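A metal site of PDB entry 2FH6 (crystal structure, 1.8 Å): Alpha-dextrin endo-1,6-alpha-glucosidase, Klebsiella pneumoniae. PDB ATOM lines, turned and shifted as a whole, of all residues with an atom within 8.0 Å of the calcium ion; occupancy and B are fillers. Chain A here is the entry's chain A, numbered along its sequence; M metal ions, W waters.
The calcium ion is bound by the side-chain carboxylate of Asp 481 (2.3 Å), the backbone carbonyl oxygen of Leu 482 (2.3 Å), water W2 (2.3 Å), water W1 (2.3 Å), the side-chain carboxylate of Glu 487 (2.4 Å) and the side-chain carboxylate of Glu 568 (2.5 Å). The calcium ion has six donor atoms within binding distance.
Of the 26 residues printed, 4 come within 4 Å of the calcium ion. The nearest printed residue that does not touch the calcium ion is Ser 388 (4.1 Å).
The backbone NH of Asp 481 is in hydrogen-bond range of the backbone carbonyl oxygen of Val 566 (2.8 Å). N of Gly 569 sits close to OE2 of Glu 487, 2.9 Å away. N of Asn 387 sits at hydrogen-bond distance from OE1 of Glu 487, 2.8 Å away. O of Asp 481 lies within hydrogen-bond range of N of His 563 (3.2 Å). OD2 of Asp 481 lies within hydrogen-bond range of OG of Ser 388 (2.5 Å). The backbone carbonyl oxygen of Asp 481 sits at hydrogen-bond distance from the backbone NH of Phe 562, 2.8 Å away. OG of Ser 570 lies within hydrogen-bond range of OE1 of Glu 568 (2.6 Å). OE1 of Glu 487 lies within salt-bridge range of NH2 of Arg 580, at 3.6 Å.
Water W2 bridges O of Val 485 (2.6 Å) and OE1 of Glu 568 (2.7 Å).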
ATOM      1  N   LEU A 384      22.127  31.279   1.102  1.00  0.00           N
ATOM      2  CA  LEU A 384      22.728  29.982   0.814  1.00  0.00           C
ATOM      3  C   LEU A 384      21.914  29.185  -0.205  1.00  0.00           C
ATOM      4  O   LEU A 384      20.758  29.509  -0.477  1.00  0.00           O
ATOM      5  CB  LEU A 384      22.800  29.161   2.092  1.00  0.00           C
ATOM      6  CG  LEU A 384      23.637  29.644   3.285  1.00  0.00           C
ATOM      7  CD1 LEU A 384      23.158  28.983   4.564  1.00  0.00           C
ATOM      8  CD2 LEU A 384      25.101  29.341   3.025  1.00  0.00           C
ATOM      9  N   SER A 385      22.532  28.145  -0.732  1.00  0.00           N
ATOM     10  CA  SER A 385      21.883  27.236  -1.659  1.00  0.00           C
ATOM     11  C   SER A 385      21.287  26.164  -0.760  1.00  0.00           C
ATOM     12  O   SER A 385      21.462  26.200   0.458  1.00  0.00           O
ATOM     13  CB  SER A 385      22.893  26.600  -2.610  1.00  0.00           C
ATOM     14  OG  SER A 385      23.802  25.742  -1.920  1.00  0.00           O
ATOM     15  N   THR A 386      20.579  25.207  -1.352  1.00  0.00           N
ATOM     16  CA  THR A 386      19.965  24.133  -0.586  1.00  0.00           C
ATOM     17  C   THR A 386      20.981  23.354   0.252  1.00  0.00           C
ATOM     18  O   THR A 386      22.023  22.932  -0.243  1.00  0.00           O
ATOM     19  CB  THR A 386      19.237  23.139  -1.510  1.00  0.00           C
ATOM     20  OG1 THR A 386      18.267  23.852  -2.296  1.00  0.00           O
ATOM     21  CG2 THR A 386      18.533  22.056  -0.687  1.00  0.00           C
ATOM     22  N   ASN A 387      20.653  23.173   1.529  1.00  0.00           N
ATOM     23  CA  ASN A 387      21.483  22.447   2.482  1.00  0.00           C
ATOM     24  C   ASN A 387      22.807  23.134   2.790  1.00  0.00           C
ATOM     25  O   ASN A 387      23.763  22.484   3.249  1.00  0.00           O
ATOM     26  CB  ASN A 387      21.745  21.006   1.992  1.00  0.00           C
ATOM     27  CG  ASN A 387      21.838  20.014   3.139  1.00  0.00           C
ATOM     28  OD1 ASN A 387      22.581  19.027   3.074  1.00  0.00           O
ATOM     29  ND2 ASN A 387      21.058  20.252   4.197  1.00  0.00           N
ATOM     30  N   SER A 388      22.863  24.435   2.531  1.00  0.00           N
ATOM     31  CA  SER A 388      24.048  25.254   2.814  1.00  0.00           C
ATOM     32  C   SER A 388      25.345  24.875   2.095  1.00  0.00           C
ATOM     33  O   SER A 388      26.417  25.184   2.581  1.00  0.00           O
ATOM     34  CB  SER A 388      24.309  25.253   4.325  1.00  0.00           C
ATOM     35  OG  SER A 388      23.115  25.381   5.073  1.00  0.00           O
ATOM     36  N   PHE A 480      18.064  30.128  12.626  1.00  0.00           N
ATOM     37  CA  PHE A 480      19.244  30.503  11.847  1.00  0.00           C
ATOM     38  C   PHE A 480      19.562  29.177  11.173  1.00  0.00           C
ATOM     39  O   PHE A 480      18.893  28.179  11.445  1.00  0.00           O
ATOM     40  CB  PHE A 480      20.390  30.941  12.762  1.00  0.00           C
ATOM     41  CG  PHE A 480      20.663  29.996  13.893  1.00  0.00           C
ATOM     42  CD1 PHE A 480      21.440  28.863  13.701  1.00  0.00           C
ATOM     43  CD2 PHE A 480      20.082  30.223  15.141  1.00  0.00           C
ATOM     44  CE1 PHE A 480      21.650  27.966  14.741  1.00  0.00           C
ATOM     45  CE2 PHE A 480      20.287  29.327  16.190  1.00  0.00           C
ATOM     46  CZ  PHE A 480      21.069  28.194  15.989  1.00  0.00           C
ATOM     47  N   ASP A 481      20.574  29.139  10.314  1.00  0.00           N
ATOM     48  CA  ASP A 481      20.888  27.914   9.596  1.00  0.00           C
ATOM     49  C   ASP A 481      21.466  26.780  10.437  1.00  0.00           C
ATOM     50  O   ASP A 481      22.658  26.761  10.744  1.00  0.00           O
ATOM     51  CB  ASP A 481      21.843  28.206   8.432  1.00  0.00           C
ATOM     52  CG  ASP A 481      22.162  26.984   7.614  1.00  0.00           C
ATOM     53  OD1 ASP A 481      21.257  26.140   7.429  1.00  0.00           O
ATOM     54  OD2 ASP A 481      23.302  26.849   7.142  1.00  0.00           O
ATOM     55  N   LEU A 482      20.607  25.831  10.800  1.00  0.00           N
ATOM     56  CA  LEU A 482      21.018  24.668  11.583  1.00  0.00           C
ATOM     57  C   LEU A 482      21.513  23.609  10.604  1.00  0.00           C
ATOM     58  O   LEU A 482      21.238  23.679   9.405  1.00  0.00           O
ATOM     59  CB  LEU A 482      19.843  24.135  12.413  1.00  0.00           C
ATOM     60  CG  LEU A 482      18.542  23.838  11.676  1.00  0.00           C
ATOM     61  CD1 LEU A 482      18.289  22.328  11.687  1.00  0.00           C
ATOM     62  CD2 LEU A 482      17.404  24.587  12.351  1.00  0.00           C
ATOM     63  N   ALA A 483      22.246  22.611  11.106  1.00  0.00           N
ATOM     64  CA  ALA A 483      22.808  21.590  10.235  1.00  0.00           C
ATOM     65  C   ALA A 483      22.140  20.230  10.294  1.00  0.00           C
ATOM     66  O   ALA A 483      22.265  19.447   9.351  1.00  0.00           O
ATOM     67  CB  ALA A 483      24.285  21.420  10.564  1.00  0.00           C
ATOM     68  N   THR A 484      21.412  19.971  11.367  1.00  0.00           N
ATOM     69  CA  THR A 484      20.800  18.667  11.595  1.00  0.00           C
ATOM     70  C   THR A 484      19.519  18.241  10.891  1.00  0.00           C
ATOM     71  O   THR A 484      18.877  17.273  11.309  1.00  0.00           O
ATOM     72  CB  THR A 484      20.660  18.443  13.094  1.00  0.00           C
ATOM     73  OG1 THR A 484      20.074  19.602  13.693  1.00  0.00           O
ATOM     74  CG2 THR A 484      22.029  18.199  13.722  1.00  0.00           C
ATOM     75  N   VAL A 485      19.151  18.940   9.824  1.00  0.00           N
ATOM     76  CA  VAL A 485      17.991  18.569   9.031  1.00  0.00           C
ATOM     77  C   VAL A 485      18.460  18.717   7.581  1.00  0.00           C
ATOM     78  O   VAL A 485      18.993  19.757   7.203  1.00  0.00           O
ATOM     79  CB  VAL A 485      16.777  19.497   9.270  1.00  0.00           C
ATOM     80  CG1 VAL A 485      15.686  19.197   8.246  1.00  0.00           C
ATOM     81  CG2 VAL A 485      16.218  19.253  10.684  1.00  0.00           C
ATOM     82  N   ASN A 486      18.288  17.665   6.782  1.00  0.00           N
ATOM     83  CA  ASN A 486      18.713  17.725   5.385  1.00  0.00           C
ATOM     84  C   ASN A 486      17.706  18.599   4.633  1.00  0.00           C
ATOM     85  O   ASN A 486      16.497  18.330   4.670  1.00  0.00           O
ATOM     86  CB  ASN A 486      18.765  16.321   4.776  1.00  0.00           C
ATOM     87  CG  ASN A 486      19.533  16.302   3.468  1.00  0.00           C
ATOM     88  OD1 ASN A 486      19.375  17.186   2.624  1.00  0.00           O
ATOM     89  ND2 ASN A 486      20.362  15.279   3.281  1.00  0.00           N
ATOM     90  N   GLU A 487      18.191  19.623   3.952  1.00  0.00           N
ATOM     91  CA  GLU A 487      17.299  20.514   3.223  1.00  0.00           C
ATOM     92  C   GLU A 487      16.891  20.011   1.842  1.00  0.00           C
ATOM     93  O   GLU A 487      16.049  20.625   1.185  1.00  0.00           O
ATOM     94  CB  GLU A 487      17.913  21.927   3.155  1.00  0.00           C
ATOM     95  CG  GLU A 487      18.121  22.531   4.539  1.00  0.00           C
ATOM     96  CD  GLU A 487      18.637  23.966   4.509  1.00  0.00           C
ATOM     97  OE1 GLU A 487      18.955  24.463   3.411  1.00  0.00           O
ATOM     98  OE2 GLU A 487      18.729  24.578   5.599  1.00  0.00           O
ATOM     99  N   ASP A 560      22.317  23.483  16.482  1.00  0.00           N
ATOM    100  CA  ASP A 560      23.457  22.976  15.718  1.00  0.00           C
ATOM    101  C   ASP A 560      23.796  23.985  14.629  1.00  0.00           C
ATOM    102  O   ASP A 560      23.442  23.793  13.471  1.00  0.00           O
ATOM    103  CB  ASP A 560      23.060  21.648  15.091  1.00  0.00           C
ATOM    104  CG  ASP A 560      22.510  20.670  16.105  1.00  0.00           C
ATOM    105  OD1 ASP A 560      21.317  20.289  16.014  1.00  0.00           O
ATOM    106  OD2 ASP A 560      23.276  20.292  17.017  1.00  0.00           O
ATOM    107  N   PRO A 561      24.502  25.063  14.985  1.00  0.00           N
ATOM    108  CA  PRO A 561      24.890  26.123  14.051  1.00  0.00           C
ATOM    109  C   PRO A 561      25.729  25.711  12.836  1.00  0.00           C
ATOM    110  O   PRO A 561      26.798  25.133  12.986  1.00  0.00           O
ATOM    111  CB  PRO A 561      25.640  27.113  14.931  1.00  0.00           C
ATOM    112  CG  PRO A 561      25.052  26.881  16.295  1.00  0.00           C
ATOM    113  CD  PRO A 561      24.965  25.381  16.344  1.00  0.00           C
ATOM    114  N   PHE A 562      25.226  26.033  11.647  1.00  0.00           N
ATOM    115  CA  PHE A 562      25.939  25.748  10.402  1.00  0.00           C
ATOM    116  C   PHE A 562      26.403  27.127   9.914  1.00  0.00           C
ATOM    117  O   PHE A 562      27.583  27.319   9.612  1.00  0.00           O
ATOM    118  CB  PHE A 562      25.008  25.076   9.403  1.00  0.00           C
ATOM    119  CG  PHE A 562      25.724  24.372   8.277  1.00  0.00           C
ATOM    120  CD1 PHE A 562      25.033  23.477   7.463  1.00  0.00           C
ATOM    121  CD2 PHE A 562      27.068  24.619   8.019  1.00  0.00           C
ATOM    122  CE1 PHE A 562      25.679  22.830   6.409  1.00  0.00           C
ATOM    123  CE2 PHE A 562      27.718  23.982   6.966  1.00  0.00           C
ATOM    124  CZ  PHE A 562      27.024  23.087   6.161  1.00  0.00           C
ATOM    125  N   HIS A 563      25.470  28.074   9.855  1.00  0.00           N
ATOM    126  CA  HIS A 563      25.754  29.470   9.477  1.00  0.00           C
ATOM    127  C   HIS A 563      24.918  30.337  10.416  1.00  0.00           C
ATOM    128  O   HIS A 563      23.689  30.184  10.499  1.00  0.00           O
ATOM    129  CB  HIS A 563      25.371  29.751   8.026  1.00  0.00           C
ATOM    130  CG  HIS A 563      26.161  28.952   7.035  1.00  0.00           C
ATOM    131  ND1 HIS A 563      27.382  29.359   6.544  1.00  0.00           N
ATOM    132  CD2 HIS A 563      25.918  27.735   6.486  1.00  0.00           C
ATOM    133  CE1 HIS A 563      27.853  28.432   5.730  1.00  0.00           C
ATOM    134  NE2 HIS A 563      26.991  27.441   5.681  1.00  0.00           N
ATOM    135  N   VAL A 566      22.026  33.335   8.437  1.00  0.00           N
ATOM    136  CA  VAL A 566      21.166  33.001   7.308  1.00  0.00           C
ATOM    137  C   VAL A 566      19.988  32.225   7.899  1.00  0.00           C
ATOM    138  O   VAL A 566      20.168  31.421   8.815  1.00  0.00           O
ATOM    139  CB  VAL A 566      21.851  32.067   6.288  1.00  0.00           C
ATOM    140  CG1 VAL A 566      20.955  31.882   5.060  1.00  0.00           C
ATOM    141  CG2 VAL A 566      23.216  32.623   5.889  1.00  0.00           C
ATOM    142  N   PRO A 567      18.764  32.483   7.421  1.00  0.00           N
ATOM    143  CA  PRO A 567      17.631  31.746   7.975  1.00  0.00           C
ATOM    144  C   PRO A 567      17.743  30.265   7.639  1.00  0.00           C
ATOM    145  O   PRO A 567      18.418  29.886   6.665  1.00  0.00           O
ATOM    146  CB  PRO A 567      16.423  32.385   7.279  1.00  0.00           C
ATOM    147  CG  PRO A 567      16.895  33.799   7.027  1.00  0.00           C
ATOM    148  CD  PRO A 567      18.308  33.580   6.554  1.00  0.00           C
ATOM    149  N   GLU A 568      17.104  29.414   8.440  1.00  0.00           N
ATOM    150  CA  GLU A 568      17.105  27.976   8.190  1.00  0.00           C
ATOM    151  C   GLU A 568      16.373  27.722   6.871  1.00  0.00           C
ATOM    152  O   GLU A 568      15.347  28.356   6.591  1.00  0.00           O
ATOM    153  CB  GLU A 568      16.406  27.255   9.354  1.00  0.00           C
ATOM    154  CG  GLU A 568      15.936  25.832   9.035  1.00  0.00           C
ATOM    155  CD  GLU A 568      17.051  24.894   8.612  1.00  0.00           C
ATOM    156  OE1 GLU A 568      16.742  23.757   8.202  1.00  0.00           O
ATOM    157  OE2 GLU A 568      18.241  25.279   8.690  1.00  0.00           O
ATOM    158  N   GLY A 569      16.884  26.794   6.078  1.00  0.00           N
ATOM    159  CA  GLY A 569      16.278  26.480   4.794  1.00  0.00           C
ATOM    160  C   GLY A 569      15.108  25.524   4.800  1.00  0.00           C
ATOM    161  O   GLY A 569      14.163  25.688   4.021  1.00  0.00           O
ATOM    162  N   SER A 570      15.135  24.521   5.679  1.00  0.00           N
ATOM    163  CA  SER A 570      14.052  23.546   5.742  1.00  0.00           C
ATOM    164  C   SER A 570      12.705  24.141   6.136  1.00  0.00           C
ATOM    165  O   SER A 570      11.656  23.557   5.866  1.00  0.00           O
ATOM    166  CB  SER A 570      14.410  22.411   6.720  1.00  0.00           C
ATOM    167  OG  SER A 570      14.346  22.868   8.060  1.00  0.00           O
ATOM    168  N   TYR A 571      12.721  25.327   6.754  1.00  0.00           N
ATOM    169  CA  TYR A 571      11.483  25.966   7.164  1.00  0.00           C
ATOM    170  C   TYR A 571      10.911  26.856   6.067  1.00  0.00           C
ATOM    171  O   TYR A 571       9.871  27.487   6.252  1.00  0.00           O
ATOM    172  CB  TYR A 571      11.681  26.799   8.444  1.00  0.00           C
ATOM    173  CG  TYR A 571      12.088  25.976   9.654  1.00  0.00           C
ATOM    174  CD1 TYR A 571      11.557  24.711   9.874  1.00  0.00           C
ATOM    175  CD2 TYR A 571      12.991  26.480  10.587  1.00  0.00           C
ATOM    176  CE1 TYR A 571      11.919  23.949  10.999  1.00  0.00           C
ATOM    177  CE2 TYR A 571      13.371  25.743  11.708  1.00  0.00           C
ATOM    178  CZ  TYR A 571      12.825  24.478  11.909  1.00  0.00           C
ATOM    179  OH  TYR A 571      13.201  23.736  13.007  1.00  0.00           O
ATOM    180  N   PRO A 575      14.168  26.085  -0.333  1.00  0.00           N
ATOM    181  CA  PRO A 575      15.478  26.303   0.303  1.00  0.00           C
ATOM    182  C   PRO A 575      16.608  26.675  -0.646  1.00  0.00           C
ATOM    183  O   PRO A 575      17.752  26.841  -0.212  1.00  0.00           O
ATOM    184  CB  PRO A 575      15.727  24.965   0.998  1.00  0.00           C
ATOM    185  CG  PRO A 575      15.186  24.004  -0.015  1.00  0.00           C
ATOM    186  CD  PRO A 575      13.880  24.637  -0.446  1.00  0.00           C
ATOM    187  N   ARG A 580      14.066  31.932   0.878  1.00  0.00           N
ATOM    188  CA  ARG A 580      13.801  31.829   2.315  1.00  0.00           C
ATOM    189  C   ARG A 580      13.833  33.169   3.050  1.00  0.00           C
ATOM    190  O   ARG A 580      13.187  33.316   4.093  1.00  0.00           O
ATOM    191  CB  ARG A 580      14.808  30.881   2.961  1.00  0.00           C
ATOM    192  CG  ARG A 580      16.183  31.495   3.144  1.00  0.00           C
ATOM    193  CD  ARG A 580      17.161  30.501   3.747  1.00  0.00           C
ATOM    194  NE  ARG A 580      17.593  29.496   2.776  1.00  0.00           N
ATOM    195  CZ  ARG A 580      18.585  28.640   2.991  1.00  0.00           C
ATOM    196  NH1 ARG A 580      19.257  28.668   4.144  1.00  0.00           N
ATOM    197  NH2 ARG A 580      18.934  27.776   2.044  1.00  0.00           N
ATOM    198  N   ARG A 616      31.654  18.137   6.955  1.00  0.00           N
ATOM    199  CA  ARG A 616      30.872  18.937   6.020  1.00  0.00           C
ATOM    200  C   ARG A 616      30.436  20.269   6.611  1.00  0.00           C
ATOM    201  O   ARG A 616      30.430  21.297   5.931  1.00  0.00           O
ATOM    202  CB  ARG A 616      29.624  18.136   5.614  1.00  0.00           C
ATOM    203  CG  ARG A 616      28.619  18.888   4.773  1.00  0.00           C
ATOM    204  CD  ARG A 616      27.358  18.037   4.568  1.00  0.00           C
ATOM    205  NE  ARG A 616      26.635  17.803   5.820  1.00  0.00           N
ATOM    206  CZ  ARG A 616      25.648  18.568   6.266  1.00  0.00           C
ATOM    207  NH1 ARG A 616      25.251  19.628   5.578  1.00  0.00           N
ATOM    208  NH2 ARG A 616      25.058  18.293   7.421  1.00  0.00           N
HETATM  209 CA    CA M   1      20.083  24.187   7.491  1.00  0.00          CA
HETATM  210  O   HOH W   1      21.641  23.204   6.037  1.00  0.00           O
HETATM  211  O   HOH W   2      18.971  22.230   8.066  1.00  0.00           O
